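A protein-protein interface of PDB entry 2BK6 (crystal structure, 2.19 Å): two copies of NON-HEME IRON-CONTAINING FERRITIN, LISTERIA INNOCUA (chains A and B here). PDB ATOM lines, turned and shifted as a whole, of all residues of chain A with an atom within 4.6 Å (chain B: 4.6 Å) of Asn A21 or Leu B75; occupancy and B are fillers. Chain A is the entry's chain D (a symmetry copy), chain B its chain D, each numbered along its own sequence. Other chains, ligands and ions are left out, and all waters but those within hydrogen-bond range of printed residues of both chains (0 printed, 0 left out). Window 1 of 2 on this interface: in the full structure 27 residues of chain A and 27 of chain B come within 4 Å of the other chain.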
ATOM      1  N   VAL A  17     -19.783 -24.565   6.815  1.00  0.00           N
ATOM      2  CA  VAL A  17     -20.759 -25.659   7.105  1.00  0.00           C
ATOM      3  C   VAL A  17     -22.171 -25.020   7.148  1.00  0.00           C
ATOM      4  O   VAL A  17     -23.110 -25.525   6.504  1.00  0.00           O
ATOM      5  CB  VAL A  17     -20.470 -26.445   8.424  1.00  0.00           C
ATOM      6  CG1 VAL A  17     -21.554 -27.518   8.699  1.00  0.00           C
ATOM      7  CG2 VAL A  17     -19.113 -27.124   8.370  1.00  0.00           C
ATOM      8  N   ALA A  18     -22.270 -23.900   7.884  1.00  0.00           N
ATOM      9  CA  ALA A  18     -23.485 -23.090   8.026  1.00  0.00           C
ATOM     10  C   ALA A  18     -23.942 -22.592   6.661  1.00  0.00           C
ATOM     11  O   ALA A  18     -25.076 -22.872   6.273  1.00  0.00           O
ATOM     12  CB  ALA A  18     -23.243 -21.919   8.992  1.00  0.00           C
ATOM     13  N   ASN A  19     -23.042 -21.916   5.933  1.00  0.00           N
ATOM     14  CA  ASN A  19     -23.307 -21.374   4.589  1.00  0.00           C
ATOM     15  C   ASN A  19     -23.801 -22.385   3.565  1.00  0.00           C
ATOM     16  O   ASN A  19     -24.812 -22.145   2.902  1.00  0.00           O
ATOM     17  CB  ASN A  19     -22.058 -20.686   4.017  1.00  0.00           C
ATOM     18  CG  ASN A  19     -21.815 -19.305   4.591  1.00  0.00           C
ATOM     19  OD1 ASN A  19     -22.643 -18.762   5.327  1.00  0.00           O
ATOM     20  ND2 ASN A  19     -20.675 -18.709   4.220  1.00  0.00           N
ATOM     21  N   LEU A  20     -23.072 -23.492   3.442  1.00  0.00           N
ATOM     22  CA  LEU A  20     -23.393 -24.549   2.469  1.00  0.00           C
ATOM     23  C   LEU A  20     -24.730 -25.210   2.716  1.00  0.00           C
ATOM     24  O   LEU A  20     -25.408 -25.553   1.762  1.00  0.00           O
ATOM     25  CB  LEU A  20     -22.249 -25.546   2.371  1.00  0.00           C
ATOM     26  CG  LEU A  20     -21.111 -25.456   1.319  1.00  0.00           C
ATOM     27  CD1 LEU A  20     -21.122 -24.364   0.231  1.00  0.00           C
ATOM     28  CD2 LEU A  20     -19.752 -25.613   2.038  1.00  0.00           C
ATOM     29  N   ASN A  21     -25.104 -25.345   3.986  1.00  0.00           N
ATOM     30  CA  ASN A  21     -26.407 -25.865   4.368  1.00  0.00           C
ATOM     31  C   ASN A  21     -27.539 -24.920   4.010  1.00  0.00           C
ATOM     32  O   ASN A  21     -28.611 -25.386   3.641  1.00  0.00           O
ATOM     33  CB  ASN A  21     -26.437 -26.264   5.825  1.00  0.00           C
ATOM     34  CG  ASN A  21     -25.932 -27.677   6.045  1.00  0.00           C
ATOM     35  OD1 ASN A  21     -26.666 -28.652   5.848  1.00  0.00           O
ATOM     36  ND2 ASN A  21     -24.698 -27.797   6.513  1.00  0.00           N
ATOM     37  N   VAL A  22     -27.301 -23.607   4.092  1.00  0.00           N
ATOM     38  CA  VAL A  22     -28.312 -22.615   3.653  1.00  0.00           C
ATOM     39  C   VAL A  22     -28.376 -22.635   2.107  1.00  0.00           C
ATOM     40  O   VAL A  22     -29.468 -22.614   1.523  1.00  0.00           O
ATOM     41  CB  VAL A  22     -28.093 -21.174   4.273  1.00  0.00           C
ATOM     42  CG1 VAL A  22     -29.131 -20.159   3.762  1.00  0.00           C
ATOM     43  CG2 VAL A  22     -28.168 -21.224   5.810  1.00  0.00           C
ATOM     44  N   PHE A  23     -27.196 -22.710   1.481  1.00  0.00           N
ATOM     45  CA  PHE A  23     -27.058 -22.720   0.034  1.00  0.00           C
ATOM     46  C   PHE A  23     -27.758 -23.902  -0.653  1.00  0.00           C
ATOM     47  O   PHE A  23     -28.466 -23.724  -1.651  1.00  0.00           O
ATOM     48  CB  PHE A  23     -25.566 -22.646  -0.340  1.00  0.00           C
ATOM     49  CG  PHE A  23     -25.303 -22.540  -1.814  1.00  0.00           C
ATOM     50  CD1 PHE A  23     -26.107 -21.728  -2.644  1.00  0.00           C
ATOM     51  CD2 PHE A  23     -24.202 -23.193  -2.372  1.00  0.00           C
ATOM     52  CE1 PHE A  23     -25.840 -21.601  -3.995  1.00  0.00           C
ATOM     53  CE2 PHE A  23     -23.921 -23.063  -3.726  1.00  0.00           C
ATOM     54  CZ  PHE A  23     -24.740 -22.274  -4.544  1.00  0.00           C
ATOM     55  N   THR A  24     -27.555 -25.087  -0.087  1.00  0.00           N
ATOM     56  CA  THR A  24     -28.090 -26.337  -0.587  1.00  0.00           C
ATOM     57  C   THR A  24     -29.651 -26.290  -0.572  1.00  0.00           C
ATOM     58  O   THR A  24     -30.312 -26.654  -1.550  1.00  0.00           O
ATOM     59  CB  THR A  24     -27.387 -27.449   0.210  1.00  0.00           C
ATOM     60  OG1 THR A  24     -26.821 -28.407  -0.679  1.00  0.00           O
ATOM     61  CG2 THR A  24     -28.156 -28.013   1.385  1.00  0.00           C
ATOM     62  N   VAL A  25     -30.192 -25.762   0.528  1.00  0.00           N
ATOM     63  CA  VAL A  25     -31.626 -25.542   0.738  1.00  0.00           C
ATOM     64  C   VAL A  25     -32.143 -24.489  -0.275  1.00  0.00           C
ATOM     65  O   VAL A  25     -33.230 -24.646  -0.830  1.00  0.00           O
ATOM     66  CB  VAL A  25     -31.883 -25.219   2.251  1.00  0.00           C
ATOM     67  CG1 VAL A  25     -33.255 -24.652   2.488  1.00  0.00           C
ATOM     68  CG2 VAL A  25     -31.685 -26.474   3.102  1.00  0.00           C
ATOM     69  N   MET A  57     -19.936 -29.442   1.562  1.00  0.00           N
ATOM     70  CA  MET A  57     -20.366 -29.227   2.945  1.00  0.00           C
ATOM     71  C   MET A  57     -19.848 -30.321   3.857  1.00  0.00           C
ATOM     72  O   MET A  57     -19.229 -30.021   4.874  1.00  0.00           O
ATOM     73  CB  MET A  57     -21.899 -29.087   3.001  1.00  0.00           C
ATOM     74  CG  MET A  57     -22.479 -28.715   4.352  1.00  0.00           C
ATOM     75  SD  MET A  57     -22.559 -30.069   5.515  1.00  0.00           S
ATOM     76  CE  MET A  57     -23.917 -31.037   4.861  1.00  0.00           C
ATOM     77  N   LEU A  75     -29.928 -27.045  12.325  1.00  0.00           N
ATOM     78  CA  LEU A  75     -30.417 -25.946  11.484  1.00  0.00           C
ATOM     79  C   LEU A  75     -30.344 -24.600  12.209  1.00  0.00           C
ATOM     80  O   LEU A  75     -30.052 -23.583  11.567  1.00  0.00           O
ATOM     81  CB  LEU A  75     -31.836 -26.197  10.966  1.00  0.00           C
ATOM     82  CG  LEU A  75     -32.137 -27.191   9.840  1.00  0.00           C
ATOM     83  CD1 LEU A  75     -32.072 -28.608  10.306  1.00  0.00           C
ATOM     84  CD2 LEU A  75     -33.536 -26.927   9.387  1.00  0.00           C
ATOM     85  N   PHE A  78     -26.848 -23.422  11.915  1.00  0.00           N
ATOM     86  CA  PHE A  78     -26.571 -22.949  10.546  1.00  0.00           C
ATOM     87  C   PHE A  78     -27.178 -21.568  10.313  1.00  0.00           C
ATOM     88  O   PHE A  78     -26.501 -20.701   9.763  1.00  0.00           O
ATOM     89  CB  PHE A  78     -27.012 -23.903   9.416  1.00  0.00           C
ATOM     90  CG  PHE A  78     -26.590 -25.342   9.581  1.00  0.00           C
ATOM     91  CD1 PHE A  78     -25.294 -25.703  10.011  1.00  0.00           C
ATOM     92  CD2 PHE A  78     -27.489 -26.355   9.210  1.00  0.00           C
ATOM     93  CE1 PHE A  78     -24.931 -27.059  10.136  1.00  0.00           C
ATOM     94  CE2 PHE A  78     -27.135 -27.705   9.318  1.00  0.00           C
ATOM     95  CZ  PHE A  78     -25.848 -28.068   9.778  1.00  0.00           C
ATOM     96  N   LEU A  79     -28.431 -21.372  10.744  1.00  0.00           N
ATOM     97  CA  LEU A  79     -29.116 -20.069  10.640  1.00  0.00           C
ATOM     98  C   LEU A  79     -28.450 -18.940  11.411  1.00  0.00           C
ATOM     99  O   LEU A  79     -28.325 -17.826  10.892  1.00  0.00           O
ATOM    100  CB  LEU A  79     -30.581 -20.173  11.071  1.00  0.00           C
ATOM    101  CG  LEU A  79     -31.620 -20.574  10.035  1.00  0.00           C
ATOM    102  CD1 LEU A  79     -32.951 -20.637  10.734  1.00  0.00           C
ATOM    103  CD2 LEU A  79     -31.681 -19.554   8.891  1.00  0.00           C
ATOM    104  N   GLU A  86     -31.227 -16.400   3.081  1.00  0.00           N
ATOM    105  CA  GLU A  86     -32.390 -17.142   2.603  1.00  0.00           C
ATOM    106  C   GLU A  86     -33.677 -16.341   2.829  1.00  0.00           C
ATOM    107  O   GLU A  86     -33.778 -15.551   3.781  1.00  0.00           O
ATOM    108  CB  GLU A  86     -32.491 -18.513   3.279  1.00  0.00           C
ATOM    109  CG  GLU A  86     -32.620 -18.510   4.828  1.00  0.00           C
ATOM    110  CD  GLU A  86     -33.041 -19.858   5.392  1.00  0.00           C
ATOM    111  OE1 GLU A  86     -32.726 -20.903   4.780  1.00  0.00           O
ATOM    112  OE2 GLU A  86     -33.710 -19.882   6.449  1.00  0.00           O
ATOM    113  N   VAL B  25     -29.823 -33.506   8.778  1.00  0.00           N
ATOM    114  CA  VAL B  25     -28.847 -32.718   9.535  1.00  0.00           C
ATOM    115  C   VAL B  25     -28.465 -33.473  10.834  1.00  0.00           C
ATOM    116  O   VAL B  25     -27.295 -33.500  11.212  1.00  0.00           O
ATOM    117  CB  VAL B  25     -29.397 -31.262   9.728  1.00  0.00           C
ATOM    118  CG1 VAL B  25     -28.631 -30.496  10.770  1.00  0.00           C
ATOM    119  CG2 VAL B  25     -29.369 -30.504   8.400  1.00  0.00           C
ATOM    120  N   THR B  74     -36.586 -23.088   3.183  1.00  0.00           N
ATOM    121  CA  THR B  74     -35.633 -22.307   3.974  1.00  0.00           C
ATOM    122  C   THR B  74     -35.481 -23.054   5.276  1.00  0.00           C
ATOM    123  O   THR B  74     -36.414 -23.762   5.683  1.00  0.00           O
ATOM    124  CB  THR B  74     -36.113 -20.851   4.285  1.00  0.00           C
ATOM    125  OG1 THR B  74     -37.376 -20.898   4.944  1.00  0.00           O
ATOM    126  CG2 THR B  74     -36.216 -19.998   3.049  1.00  0.00           C
ATOM    127  N   LEU B  75     -34.319 -22.899   5.923  1.00  0.00           N
ATOM    128  CA  LEU B  75     -34.050 -23.514   7.228  1.00  0.00           C
ATOM    129  C   LEU B  75     -34.981 -22.970   8.316  1.00  0.00           C
ATOM    130  O   LEU B  75     -35.388 -23.735   9.200  1.00  0.00           O
ATOM    131  CB  LEU B  75     -32.588 -23.361   7.653  1.00  0.00           C
ATOM    132  CG  LEU B  75     -31.459 -24.190   7.031  1.00  0.00           C
ATOM    133  CD1 LEU B  75     -31.097 -23.713   5.663  1.00  0.00           C
ATOM    134  CD2 LEU B  75     -30.258 -24.016   7.903  1.00  0.00           C
ATOM    135  N   LYS B  76     -35.302 -21.670   8.225  1.00  0.00           N
ATOM    136  CA  LYS B  76     -36.242 -20.966   9.121  1.00  0.00           C
ATOM    137  C   LYS B  76     -37.592 -21.685   9.104  1.00  0.00           C
ATOM    138  O   LYS B  76     -38.103 -22.036  10.162  1.00  0.00           O
ATOM    139  CB  LYS B  76     -36.383 -19.486   8.720  1.00  0.00           C
ATOM    140  CG  LYS B  76     -37.288 -18.633   9.641  1.00  0.00           C
ATOM    141  CD  LYS B  76     -37.629 -17.326   8.943  1.00  0.00           C
ATOM    142  CE  LYS B  76     -38.581 -16.442   9.739  1.00  0.00           C
ATOM    143  NZ  LYS B  76     -37.893 -15.663  10.802  1.00  0.00           N
ATOM    144  N   GLU B  77     -38.126 -21.927   7.898  1.00  0.00           N
ATOM    145  CA  GLU B  77     -39.384 -22.672   7.699  1.00  0.00           C
ATOM    146  C   GLU B  77     -39.307 -24.104   8.218  1.00  0.00           C
ATOM    147  O   GLU B  77     -40.264 -24.564   8.836  1.00  0.00           O
ATOM    148  CB  GLU B  77     -39.811 -22.691   6.244  1.00  0.00           C
ATOM    149  CG  GLU B  77     -40.422 -21.414   5.731  1.00  0.00           C
ATOM    150  CD  GLU B  77     -40.568 -21.408   4.224  1.00  0.00           C
ATOM    151  OE1 GLU B  77     -39.565 -21.603   3.507  1.00  0.00           O
ATOM    152  OE2 GLU B  77     -41.688 -21.168   3.738  1.00  0.00           O
ATOM    153  N   PHE B  78     -38.182 -24.799   7.986  1.00  0.00           N
ATOM    154  CA  PHE B  78     -38.047 -26.181   8.483  1.00  0.00           C
ATOM    155  C   PHE B  78     -38.052 -26.213  10.009  1.00  0.00           C
ATOM    156  O   PHE B  78     -38.742 -27.050  10.588  1.00  0.00           O
ATOM    157  CB  PHE B  78     -36.821 -26.955   7.956  1.00  0.00           C
ATOM    158  CG  PHE B  78     -36.614 -26.901   6.462  1.00  0.00           C
ATOM    159  CD1 PHE B  78     -37.680 -27.045   5.548  1.00  0.00           C
ATOM    160  CD2 PHE B  78     -35.305 -26.792   5.966  1.00  0.00           C
ATOM    161  CE1 PHE B  78     -37.445 -27.007   4.158  1.00  0.00           C
ATOM    162  CE2 PHE B  78     -35.057 -26.766   4.589  1.00  0.00           C
ATOM    163  CZ  PHE B  78     -36.129 -26.879   3.672  1.00  0.00           C
ATOM    164  N   LEU B  79     -37.302 -25.301  10.641  1.00  0.00           N
ATOM    165  CA  LEU B  79     -37.264 -25.179  12.112  1.00  0.00           C
ATOM    166  C   LEU B  79     -38.599 -24.835  12.754  1.00  0.00           C
ATOM    167  O   LEU B  79     -38.963 -25.423  13.777  1.00  0.00           O
ATOM    168  CB  LEU B  79     -36.215 -24.159  12.560  1.00  0.00           C
ATOM    169  CG  LEU B  79     -34.782 -24.625  12.763  1.00  0.00           C
ATOM    170  CD1 LEU B  79     -33.968 -23.423  13.157  1.00  0.00           C
ATOM    171  CD2 LEU B  79     -34.699 -25.692  13.863  1.00  0.00           C
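The side-chain carboxylate of Glu B77 is in hydrogen-bond range of the side-chain hydroxyl of Thr B74, at 2.7 Å. O of Val A17 is in hydrogen-bond range of ND2 of Asn A21 (2.8 Å). The side-chain amide nitrogen of Asn A21 lies close to the side-chain sulfur of Met A57 (3.3 Å).
Of the 14 printed residues of chain A, 7 touch a printed residue of chain B. Of the 7 printed residues of chain B, 6 touch a printed residue of chain A. Among the printed residues, 17 pairs touch across the chains.
Val A25 touches Phe B78, and with the chains exchanged Phe A78 touches Val B25. Leu A75 touches its own counterpart, Leu B75. Leu A75 touches Phe B78, and with the chains exchanged Phe A78 touches Leu B75. Leu A75 touches Leu B79, and with the chains exchanged Leu A79 touches Leu B75. Of the 17 pairs that touch across the chains among the printed residues, 10 have their exchanged pair printed and touching as well.
N of Leu B75 sits at hydrogen-bond distance from OE1 of Glu A86 (2.8 Å). The backbone NH (N) of Lys B76 sits at hydrogen-bond distance from the side-chain carboxylate (OE2) of Glu A86 (3.0 Å).
Among the printed residues, merely in contact across the chains: Asn A21 with Leu B75 (3.6 Å), Val A22 with Leu B75 (3.6 Å), Val A25 with Thr B74 (3.7 Å), Val A25 with Leu B75 (3.8 Å), Val A25 with Phe B78 (3.5 Å), Leu A75 with Val B25 (3.8 Å), Leu A75 with Leu B75 (3.7 Å), Leu A75 with Phe B78 (3.6 Å), Leu A75 with Leu B79 (3.8 Å), Phe A78 with Val B25 (3.5 Å), Phe A78 with Leu B75 (3.6 Å), Leu A79 with Leu B75 (3.8 Å), Leu A79 with Lys B76 (3.6 Å), Leu A79 with Leu B79 (3.8 Å) and Glu A86 with Thr B74 (3.3 Å).
Of chain B, only Leu B75 (3.6 Å) comes within 4 Å of Asn A21. Of chain A, only Asn A21 (3.6 Å), Val A22 (3.6 Å), Val A25 (3.8 Å), Leu A75 (3.7 Å), Phe A78 (3.6 Å), Leu A79 (3.8 Å) and Glu A86 (2.8 Å) come within 4 Å of Leu B75. Of the printed residues of chain A, Val B25 touches Leu A75 (3.8 Å) and Phe A78 (3.5 Å). Printed residues of chain A within 4 Å of Thr B74: Val A25 and Glu A86. Printed residues of chain A within 4 Å of Leu B79: Leu A75 (3.8 Å) and Leu A79 (3.8 Å). Of the printed residues of chain B, Leu A79 touches Leu B75 (3.8 Å), Lys B76 (3.6 Å) and Leu B79 (3.8 Å). The nearest printed residue of chain A that does not touch Thr B74 is Leu A75 (5.7 Å).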
